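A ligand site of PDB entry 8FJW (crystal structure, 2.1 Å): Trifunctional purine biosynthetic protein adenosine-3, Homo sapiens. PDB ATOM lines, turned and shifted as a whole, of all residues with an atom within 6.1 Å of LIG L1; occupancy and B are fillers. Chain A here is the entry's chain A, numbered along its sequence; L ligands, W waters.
Residues that only touch LIG L1: Leu 86 (3.6 Å), Phe 89 (3.9 Å), Val 98 (3.6 Å), Asn 107 (3.3 Å), Gly 118 (3.9 Å), Ser 119 (3.8 Å), Val 140 (3.6 Å) and Val 144 (3.9 Å).
Hydrophobic or aromatic side chains that line LIG L1: Leu 86, Met 90, Ile 92, Leu 93, Val 98, Val 140 and Val 144.
Within 4 Å of LIG L1: Arg 65, Leu 86, Phe 89, Met 90, Arg 91, Ile 92, Leu 93, Val 98, Asn 107, Gly 118, Ser 119, Val 140, Ala 141, Glu 142 and Val 144.
The nearest printed residue that does not touch LIG L1 is His 138 (4.1 Å).
Water W1 lies within hydrogen-bond range of an oxygen (O1) of LIG L1 (3.0 Å) and the backbone NH of Ala 141 (3.0 Å).
The guanidinium group of Arg 65 sits at hydrogen-bond distance from the backbone carbonyl oxygen of Ile 92, 3.0 Å away.
A ring nitrogen (NE2) of His 138 sits at hydrogen-bond distance from the side-chain amide nitrogen (ND2) of Asn 107 (3.0 Å).
The guanidinium group (NH2) of Arg 65 is in salt-bridge range of an oxygen (O5) of LIG L1, 2.6 Å away.
A nitrogen (N1) of LIG L1 is in hydrogen-bond range of the backbone NH (N) of Leu 93.
The backbone carbonyl oxygen (O) of Leu 93 is in hydrogen-bond range of a nitrogen (N2) of LIG L1 (3.3 Å).
An oxygen (O6) of LIG L1 lies within salt-bridge range of the guanidinium group (NE) of Arg 91.
N of Ile 92 sits at hydrogen-bond distance from O6 of LIG L1.
O of Met 90 sits close to N3 of LIG L1, at 3.5 Å.
O of Glu 142 is in hydrogen-bond range of N2 of LIG L1 (3.4 Å).
A nitrogen (N4) of LIG L1 sits at hydrogen-bond distance from the backbone carbonyl oxygen of Ala 141.
A ring nitrogen (ND1) of His 109 sits at hydrogen-bond distance from a nitrogen (N2) of LG2 L2, at 3.1 Å.
O of Ile 108 is in hydrogen-bond range of N2 of LG2 L2.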
ATOM      1  N   ARG A  65      16.663   5.817 -26.990  1.00  0.00           N
ATOM      2  CA  ARG A  65      17.052   6.914 -26.103  1.00  0.00           C
ATOM      3  C   ARG A  65      15.956   7.962 -26.010  1.00  0.00           C
ATOM      4  O   ARG A  65      15.611   8.423 -24.916  1.00  0.00           O
ATOM      5  CB  ARG A  65      18.366   7.542 -26.574  1.00  0.00           C
ATOM      6  CG  ARG A  65      19.616   6.733 -26.280  1.00  0.00           C
ATOM      7  CD  ARG A  65      20.847   7.619 -26.387  1.00  0.00           C
ATOM      8  NE  ARG A  65      22.080   6.840 -26.574  1.00  0.00           N
ATOM      9  CZ  ARG A  65      22.885   6.457 -25.585  1.00  0.00           C
ATOM     10  NH1 ARG A  65      22.600   6.763 -24.334  1.00  0.00           N
ATOM     11  NH2 ARG A  65      23.981   5.767 -25.867  1.00  0.00           N
ATOM     12  N   LEU A  86      23.313  17.144 -13.812  1.00  0.00           N
ATOM     13  CA  LEU A  86      23.822  15.797 -14.028  1.00  0.00           C
ATOM     14  C   LEU A  86      24.954  15.555 -13.046  1.00  0.00           C
ATOM     15  O   LEU A  86      26.038  16.143 -13.185  1.00  0.00           O
ATOM     16  CB  LEU A  86      24.275  15.614 -15.473  1.00  0.00           C
ATOM     17  CG  LEU A  86      23.238  15.954 -16.546  1.00  0.00           C
ATOM     18  CD1 LEU A  86      23.767  15.639 -17.933  1.00  0.00           C
ATOM     19  CD2 LEU A  86      21.932  15.223 -16.276  1.00  0.00           C
ATOM     20  N   PHE A  89      25.578  11.125 -13.795  1.00  0.00           N
ATOM     21  CA  PHE A  89      24.628  10.497 -14.702  1.00  0.00           C
ATOM     22  C   PHE A  89      25.384   9.958 -15.900  1.00  0.00           C
ATOM     23  O   PHE A  89      25.891  10.724 -16.725  1.00  0.00           O
ATOM     24  CB  PHE A  89      23.552  11.495 -15.113  1.00  0.00           C
ATOM     25  CG  PHE A  89      22.378  10.881 -15.825  1.00  0.00           C
ATOM     26  CD1 PHE A  89      21.498  10.062 -15.146  1.00  0.00           C
ATOM     27  CD2 PHE A  89      22.148  11.140 -17.160  1.00  0.00           C
ATOM     28  CE1 PHE A  89      20.412   9.497 -15.785  1.00  0.00           C
ATOM     29  CE2 PHE A  89      21.068  10.587 -17.817  1.00  0.00           C
ATOM     30  CZ  PHE A  89      20.194   9.764 -17.121  1.00  0.00           C
ATOM     31  N   MET A  90      25.466   8.624 -16.018  1.00  0.00           N
ATOM     32  CA  MET A  90      26.281   7.962 -17.037  1.00  0.00           C
ATOM     33  C   MET A  90      25.427   7.464 -18.196  1.00  0.00           C
ATOM     34  O   MET A  90      25.572   6.327 -18.650  1.00  0.00           O
ATOM     35  CB  MET A  90      27.055   6.812 -16.403  1.00  0.00           C
ATOM     36  CG  MET A  90      27.905   7.199 -15.217  1.00  0.00           C
ATOM     37  SD  MET A  90      29.164   8.433 -15.625  1.00  0.00           S
ATOM     38  CE  MET A  90      30.026   8.539 -14.058  1.00  0.00           C
ATOM     39  N   ARG A  91      24.534   8.301 -18.710  1.00  0.00           N
ATOM     40  CA  ARG A  91      23.686   7.933 -19.835  1.00  0.00           C
ATOM     41  C   ARG A  91      23.596   9.132 -20.762  1.00  0.00           C
ATOM     42  O   ARG A  91      23.047  10.172 -20.387  1.00  0.00           O
ATOM     43  CB  ARG A  91      22.292   7.501 -19.365  1.00  0.00           C
ATOM     44  CG  ARG A  91      21.572   6.571 -20.318  1.00  0.00           C
ATOM     45  CD  ARG A  91      22.247   5.218 -20.362  1.00  0.00           C
ATOM     46  NE  ARG A  91      21.857   4.439 -21.529  1.00  0.00           N
ATOM     47  CZ  ARG A  91      22.379   3.254 -21.841  1.00  0.00           C
ATOM     48  NH1 ARG A  91      21.976   2.605 -22.924  1.00  0.00           N
ATOM     49  NH2 ARG A  91      23.314   2.717 -21.062  1.00  0.00           N
ATOM     50  N   ILE A  92      24.146   9.000 -21.966  1.00  0.00           N
ATOM     51  CA  ILE A  92      24.145  10.123 -22.900  1.00  0.00           C
ATOM     52  C   ILE A  92      22.720  10.483 -23.271  1.00  0.00           C
ATOM     53  O   ILE A  92      21.870   9.598 -23.492  1.00  0.00           O
ATOM     54  CB  ILE A  92      24.991   9.793 -24.142  1.00  0.00           C
ATOM     55  CG1 ILE A  92      26.436   9.507 -23.744  1.00  0.00           C
ATOM     56  CG2 ILE A  92      24.940  10.952 -25.130  1.00  0.00           C
ATOM     57  CD1 ILE A  92      27.096  10.646 -22.983  1.00  0.00           C
ATOM     58  N   LEU A  93      22.452  11.773 -23.356  1.00  0.00           N
ATOM     59  CA  LEU A  93      21.110  12.293 -23.608  1.00  0.00           C
ATOM     60  C   LEU A  93      20.953  12.659 -25.074  1.00  0.00           C
ATOM     61  O   LEU A  93      21.905  13.091 -25.729  1.00  0.00           O
ATOM     62  CB  LEU A  93      20.836  13.519 -22.724  1.00  0.00           C
ATOM     63  CG  LEU A  93      20.959  13.266 -21.221  1.00  0.00           C
ATOM     64  CD1 LEU A  93      21.316  14.541 -20.488  1.00  0.00           C
ATOM     65  CD2 LEU A  93      19.663  12.675 -20.671  1.00  0.00           C
ATOM     66  N   SER A  94      19.740  12.485 -25.581  1.00  0.00           N
ATOM     67  CA  SER A  94      19.475  12.707 -26.997  1.00  0.00           C
ATOM     68  C   SER A  94      19.463  14.198 -27.327  1.00  0.00           C
ATOM     69  O   SER A  94      19.287  15.056 -26.458  1.00  0.00           O
ATOM     70  CB  SER A  94      18.141  12.075 -27.393  1.00  0.00           C
ATOM     71  OG  SER A  94      17.061  12.634 -26.664  1.00  0.00           O
ATOM     72  N   GLY A  95      19.636  14.489 -28.619  1.00  0.00           N
ATOM     73  CA  GLY A  95      19.705  15.844 -29.101  1.00  0.00           C
ATOM     74  C   GLY A  95      18.502  16.693 -28.747  1.00  0.00           C
ATOM     75  O   GLY A  95      18.639  17.829 -28.277  1.00  0.00           O
ATOM     76  N   VAL A  98      18.559  17.523 -25.017  1.00  0.00           N
ATOM     77  CA  VAL A  98      19.597  18.515 -24.782  1.00  0.00           C
ATOM     78  C   VAL A  98      19.179  19.861 -25.356  1.00  0.00           C
ATOM     79  O   VAL A  98      19.452  20.922 -24.787  1.00  0.00           O
ATOM     80  CB  VAL A  98      20.940  18.041 -25.365  1.00  0.00           C
ATOM     81  CG1 VAL A  98      21.980  19.152 -25.260  1.00  0.00           C
ATOM     82  CG2 VAL A  98      21.412  16.788 -24.650  1.00  0.00           C
ATOM     83  N   ASN A 107      26.503  19.931 -15.840  1.00  0.00           N
ATOM     84  CA  ASN A 107      27.183  18.648 -15.697  1.00  0.00           C
ATOM     85  C   ASN A 107      28.544  18.883 -15.051  1.00  0.00           C
ATOM     86  O   ASN A 107      29.215  19.873 -15.339  1.00  0.00           O
ATOM     87  CB  ASN A 107      27.339  17.946 -17.049  1.00  0.00           C
ATOM     88  CG  ASN A 107      28.138  16.661 -16.957  1.00  0.00           C
ATOM     89  OD1 ASN A 107      27.690  15.676 -16.381  1.00  0.00           O
ATOM     90  ND2 ASN A 107      29.340  16.674 -17.533  1.00  0.00           N
ATOM     91  N   ILE A 108      28.935  17.976 -14.169  1.00  0.00           N
ATOM     92  CA  ILE A 108      30.251  17.979 -13.542  1.00  0.00           C
ATOM     93  C   ILE A 108      31.111  16.932 -14.225  1.00  0.00           C
ATOM     94  O   ILE A 108      30.697  15.762 -14.346  1.00  0.00           O
ATOM     95  CB  ILE A 108      30.147  17.726 -12.023  1.00  0.00           C
ATOM     96  CG1 ILE A 108      31.531  17.714 -11.360  1.00  0.00           C
ATOM     97  CG2 ILE A 108      29.440  16.408 -11.753  1.00  0.00           C
ATOM     98  CD1 ILE A 108      32.218  19.059 -11.346  1.00  0.00           C
ATOM     99  N   HIS A 109      32.286  17.329 -14.684  1.00  0.00           N
ATOM    100  CA  HIS A 109      33.200  16.425 -15.369  1.00  0.00           C
ATOM    101  C   HIS A 109      34.552  16.428 -14.660  1.00  0.00           C
ATOM    102  O   HIS A 109      35.094  17.505 -14.386  1.00  0.00           O
ATOM    103  CB  HIS A 109      33.373  16.831 -16.849  1.00  0.00           C
ATOM    104  CG  HIS A 109      34.185  15.868 -17.649  1.00  0.00           C
ATOM    105  ND1 HIS A 109      33.754  14.596 -17.950  1.00  0.00           N
ATOM    106  CD2 HIS A 109      35.413  15.992 -18.221  1.00  0.00           C
ATOM    107  CE1 HIS A 109      34.668  13.977 -18.674  1.00  0.00           C
ATOM    108  NE2 HIS A 109      35.690  14.802 -18.852  1.00  0.00           N
ATOM    109  N   GLY A 118      35.108  12.506 -22.185  1.00  0.00           N
ATOM    110  CA  GLY A 118      34.695  11.108 -22.207  1.00  0.00           C
ATOM    111  C   GLY A 118      34.568  10.490 -20.827  1.00  0.00           C
ATOM    112  O   GLY A 118      34.631  11.154 -19.789  1.00  0.00           O
ATOM    113  N   SER A 119      34.419   9.167 -20.838  1.00  0.00           N
ATOM    114  CA  SER A 119      33.946   8.434 -19.668  1.00  0.00           C
ATOM    115  C   SER A 119      35.044   8.096 -18.665  1.00  0.00           C
ATOM    116  O   SER A 119      34.722   7.808 -17.507  1.00  0.00           O
ATOM    117  CB  SER A 119      33.256   7.157 -20.114  1.00  0.00           C
ATOM    118  OG  SER A 119      34.132   6.352 -20.890  1.00  0.00           O
ATOM    119  N   HIS A 138      29.912  22.552 -16.498  1.00  0.00           N
ATOM    120  CA  HIS A 138      29.619  23.162 -17.782  1.00  0.00           C
ATOM    121  C   HIS A 138      28.163  22.946 -18.155  1.00  0.00           C
ATOM    122  O   HIS A 138      27.518  21.996 -17.700  1.00  0.00           O
ATOM    123  CB  HIS A 138      30.517  22.588 -18.890  1.00  0.00           C
ATOM    124  CG  HIS A 138      30.297  21.128 -19.149  1.00  0.00           C
ATOM    125  ND1 HIS A 138      29.432  20.662 -20.120  1.00  0.00           N
ATOM    126  CD2 HIS A 138      30.828  20.029 -18.548  1.00  0.00           C
ATOM    127  CE1 HIS A 138      29.450  19.341 -20.114  1.00  0.00           C
ATOM    128  NE2 HIS A 138      30.281  18.937 -19.176  1.00  0.00           N
ATOM    129  N   VAL A 140      25.412  21.578 -20.588  1.00  0.00           N
ATOM    130  CA  VAL A 140      25.400  20.400 -21.449  1.00  0.00           C
ATOM    131  C   VAL A 140      24.973  20.824 -22.850  1.00  0.00           C
ATOM    132  O   VAL A 140      23.897  21.410 -23.037  1.00  0.00           O
ATOM    133  CB  VAL A 140      24.476  19.306 -20.896  1.00  0.00           C
ATOM    134  CG1 VAL A 140      24.348  18.180 -21.899  1.00  0.00           C
ATOM    135  CG2 VAL A 140      25.014  18.790 -19.568  1.00  0.00           C
ATOM    136  N   ALA A 141      25.810  20.536 -23.833  1.00  0.00           N
ATOM    137  CA  ALA A 141      25.522  20.754 -25.242  1.00  0.00           C
ATOM    138  C   ALA A 141      25.443  19.413 -25.958  1.00  0.00           C
ATOM    139  O   ALA A 141      25.808  18.376 -25.419  1.00  0.00           O
ATOM    140  CB  ALA A 141      26.582  21.657 -25.881  1.00  0.00           C
ATOM    141  N   GLU A 142      24.943  19.454 -27.198  1.00  0.00           N
ATOM    142  CA  GLU A 142      24.771  18.210 -27.957  1.00  0.00           C
ATOM    143  C   GLU A 142      26.101  17.492 -28.139  1.00  0.00           C
ATOM    144  O   GLU A 142      26.206  16.288 -27.865  1.00  0.00           O
ATOM    145  CB  GLU A 142      24.107  18.511 -29.298  1.00  0.00           C
ATOM    146  CG  GLU A 142      22.628  18.138 -29.343  1.00  0.00           C
ATOM    147  CD  GLU A 142      21.863  18.891 -30.405  1.00  0.00           C
ATOM    148  OE1 GLU A 142      21.965  20.136 -30.458  1.00  0.00           O
ATOM    149  OE2 GLU A 142      21.139  18.237 -31.191  1.00  0.00           O
ATOM    150  N   ASP A 143      27.117  18.208 -28.597  1.00  0.00           N
ATOM    151  CA  ASP A 143      28.475  17.676 -28.654  1.00  0.00           C
ATOM    152  C   ASP A 143      29.263  18.222 -27.467  1.00  0.00           C
ATOM    153  O   ASP A 143      29.318  19.430 -27.252  1.00  0.00           O
ATOM    154  CB  ASP A 143      29.161  18.054 -29.967  1.00  0.00           C
ATOM    155  CG  ASP A 143      29.157  19.546 -30.224  1.00  0.00           C
ATOM    156  OD1 ASP A 143      28.121  20.196 -29.973  1.00  0.00           O
ATOM    157  OD2 ASP A 143      30.201  20.077 -30.679  1.00  0.00           O
ATOM    158  N   VAL A 144      29.885  17.315 -26.703  1.00  0.00           N
ATOM    159  CA  VAL A 144      30.607  17.700 -25.502  1.00  0.00           C
ATOM    160  C   VAL A 144      31.728  18.699 -25.782  1.00  0.00           C
ATOM    161  O   VAL A 144      32.321  19.231 -24.849  1.00  0.00           O
ATOM    162  CB  VAL A 144      31.178  16.454 -24.799  1.00  0.00           C
ATOM    163  CG1 VAL A 144      31.374  16.716 -23.307  1.00  0.00           C
ATOM    164  CG2 VAL A 144      30.261  15.249 -25.020  1.00  0.00           C
HETATM  165  C1  LIG L   1      26.052  14.368 -21.439  1.00  0.00           C
HETATM  166  C2  LIG L   1      24.569  12.816 -20.785  1.00  0.00           C
HETATM  167  C3  LIG L   1      25.501  13.060 -19.779  1.00  0.00           C
HETATM  168  N1  LIG L   1      24.453  13.921 -23.104  1.00  0.00           N
HETATM  169  C4  LIG L   1      25.041  14.808 -23.904  1.00  0.00           C
HETATM  170  C5  LIG L   1      26.649  15.315 -22.318  1.00  0.00           C
HETATM  171  C6  LIG L   1      24.941  13.679 -21.860  1.00  0.00           C
HETATM  172  C7  LIG L   1      29.303   8.140 -21.250  1.00  0.00           C
HETATM  173  C8  LIG L   1      30.326   8.856 -21.860  1.00  0.00           C
HETATM  174  C9  LIG L   1      28.650   8.652 -20.150  1.00  0.00           C
HETATM  175  C10 LIG L   1      30.702  10.090 -21.364  1.00  0.00           C
HETATM  176  C11 LIG L   1      29.020   9.884 -19.646  1.00  0.00           C
HETATM  177  C12 LIG L   1      28.863   6.781 -21.786  1.00  0.00           C
HETATM  178  C13 LIG L   1      27.007   5.096 -22.060  1.00  0.00           C
HETATM  179  C14 LIG L   1      26.642   4.207 -20.869  1.00  0.00           C
HETATM  180  C15 LIG L   1      27.712   4.298 -19.774  1.00  0.00           C
HETATM  181  C16 LIG L   1      27.610   3.187 -18.748  1.00  0.00           C
HETATM  182  C17 LIG L   1      25.771   5.347 -22.911  1.00  0.00           C
HETATM  183  C18 LIG L   1      27.480  14.503 -19.417  1.00  0.00           C
HETATM  184  C19 LIG L   1      28.793  13.891 -19.910  1.00  0.00           C
HETATM  185  C20 LIG L   1      29.136  12.618 -19.147  1.00  0.00           C
HETATM  186  C21 LIG L   1      30.417  11.961 -19.667  1.00  0.00           C
HETATM  187  C22 LIG L   1      30.043  10.600 -20.256  1.00  0.00           C
HETATM  188  F1  LIG L   1      30.961   8.343 -22.961  1.00  0.00           F
HETATM  189  N2  LIG L   1      24.482  15.040 -25.222  1.00  0.00           N
HETATM  190  N3  LIG L   1      27.487   6.367 -21.574  1.00  0.00           N
HETATM  191  N4  LIG L   1      26.114  15.497 -23.514  1.00  0.00           N
HETATM  192  N5  LIG L   1      26.358  13.980 -20.178  1.00  0.00           N
HETATM  193  O1  LIG L   1      27.772  16.033 -21.918  1.00  0.00           O
HETATM  194  O2  LIG L   1      29.621   6.074 -22.360  1.00  0.00           O
HETATM  195  O3  LIG L   1      27.219   2.045 -19.107  1.00  0.00           O
HETATM  196  O4  LIG L   1      27.920   3.401 -17.551  1.00  0.00           O
HETATM  197  O5  LIG L   1      25.708   4.902 -24.090  1.00  0.00           O
HETATM  198  O6  LIG L   1      24.810   6.012 -22.448  1.00  0.00           O
HETATM  199  C1  LG2 L   2      31.946  12.249 -10.480  1.00  0.00           C
HETATM  200  O1  LG2 L   2      33.289  12.199 -10.021  1.00  0.00           O
HETATM  201  C2  LG2 L   2      31.820  12.849 -11.884  1.00  0.00           C
HETATM  202  O2  LG2 L   2      32.836  13.765 -12.222  1.00  0.00           O
HETATM  203  C3  LG2 L   2      31.829  11.600 -12.778  1.00  0.00           C
HETATM  204  O3  LG2 L   2      31.187  10.567 -11.990  1.00  0.00           O
HETATM  205  C4  LG2 L   2      31.405  10.821 -10.589  1.00  0.00           C
HETATM  206  C5  LG2 L   2      30.134  10.600  -9.792  1.00  0.00           C
HETATM  207  O4  LG2 L   2      30.400  10.808  -8.406  1.00  0.00           O
HETATM  208  N1  LG2 L   2      31.170  11.784 -14.046  1.00  0.00           N
HETATM  209  C6  LG2 L   2      31.823  11.580 -15.191  1.00  0.00           C
HETATM  210  O5  LG2 L   2      32.955  11.117 -15.264  1.00  0.00           O
HETATM  211  C7  LG2 L   2      31.077  11.971 -16.449  1.00  0.00           C
HETATM  212  N2  LG2 L   2      31.149  13.409 -16.689  1.00  0.00           N
HETATM  213  P1  LG2 L   2      29.184  10.820  -7.342  1.00  0.00           P
HETATM  214  O6  LG2 L   2      28.715  12.249  -7.399  1.00  0.00           O
HETATM  215  O7  LG2 L   2      29.824  10.413  -6.042  1.00  0.00           O
HETATM  216  O8  LG2 L   2      28.174   9.836  -7.897  1.00  0.00           O
HETATM  217  O   HOH W   1      28.184  18.715 -23.254  1.00  0.00           O
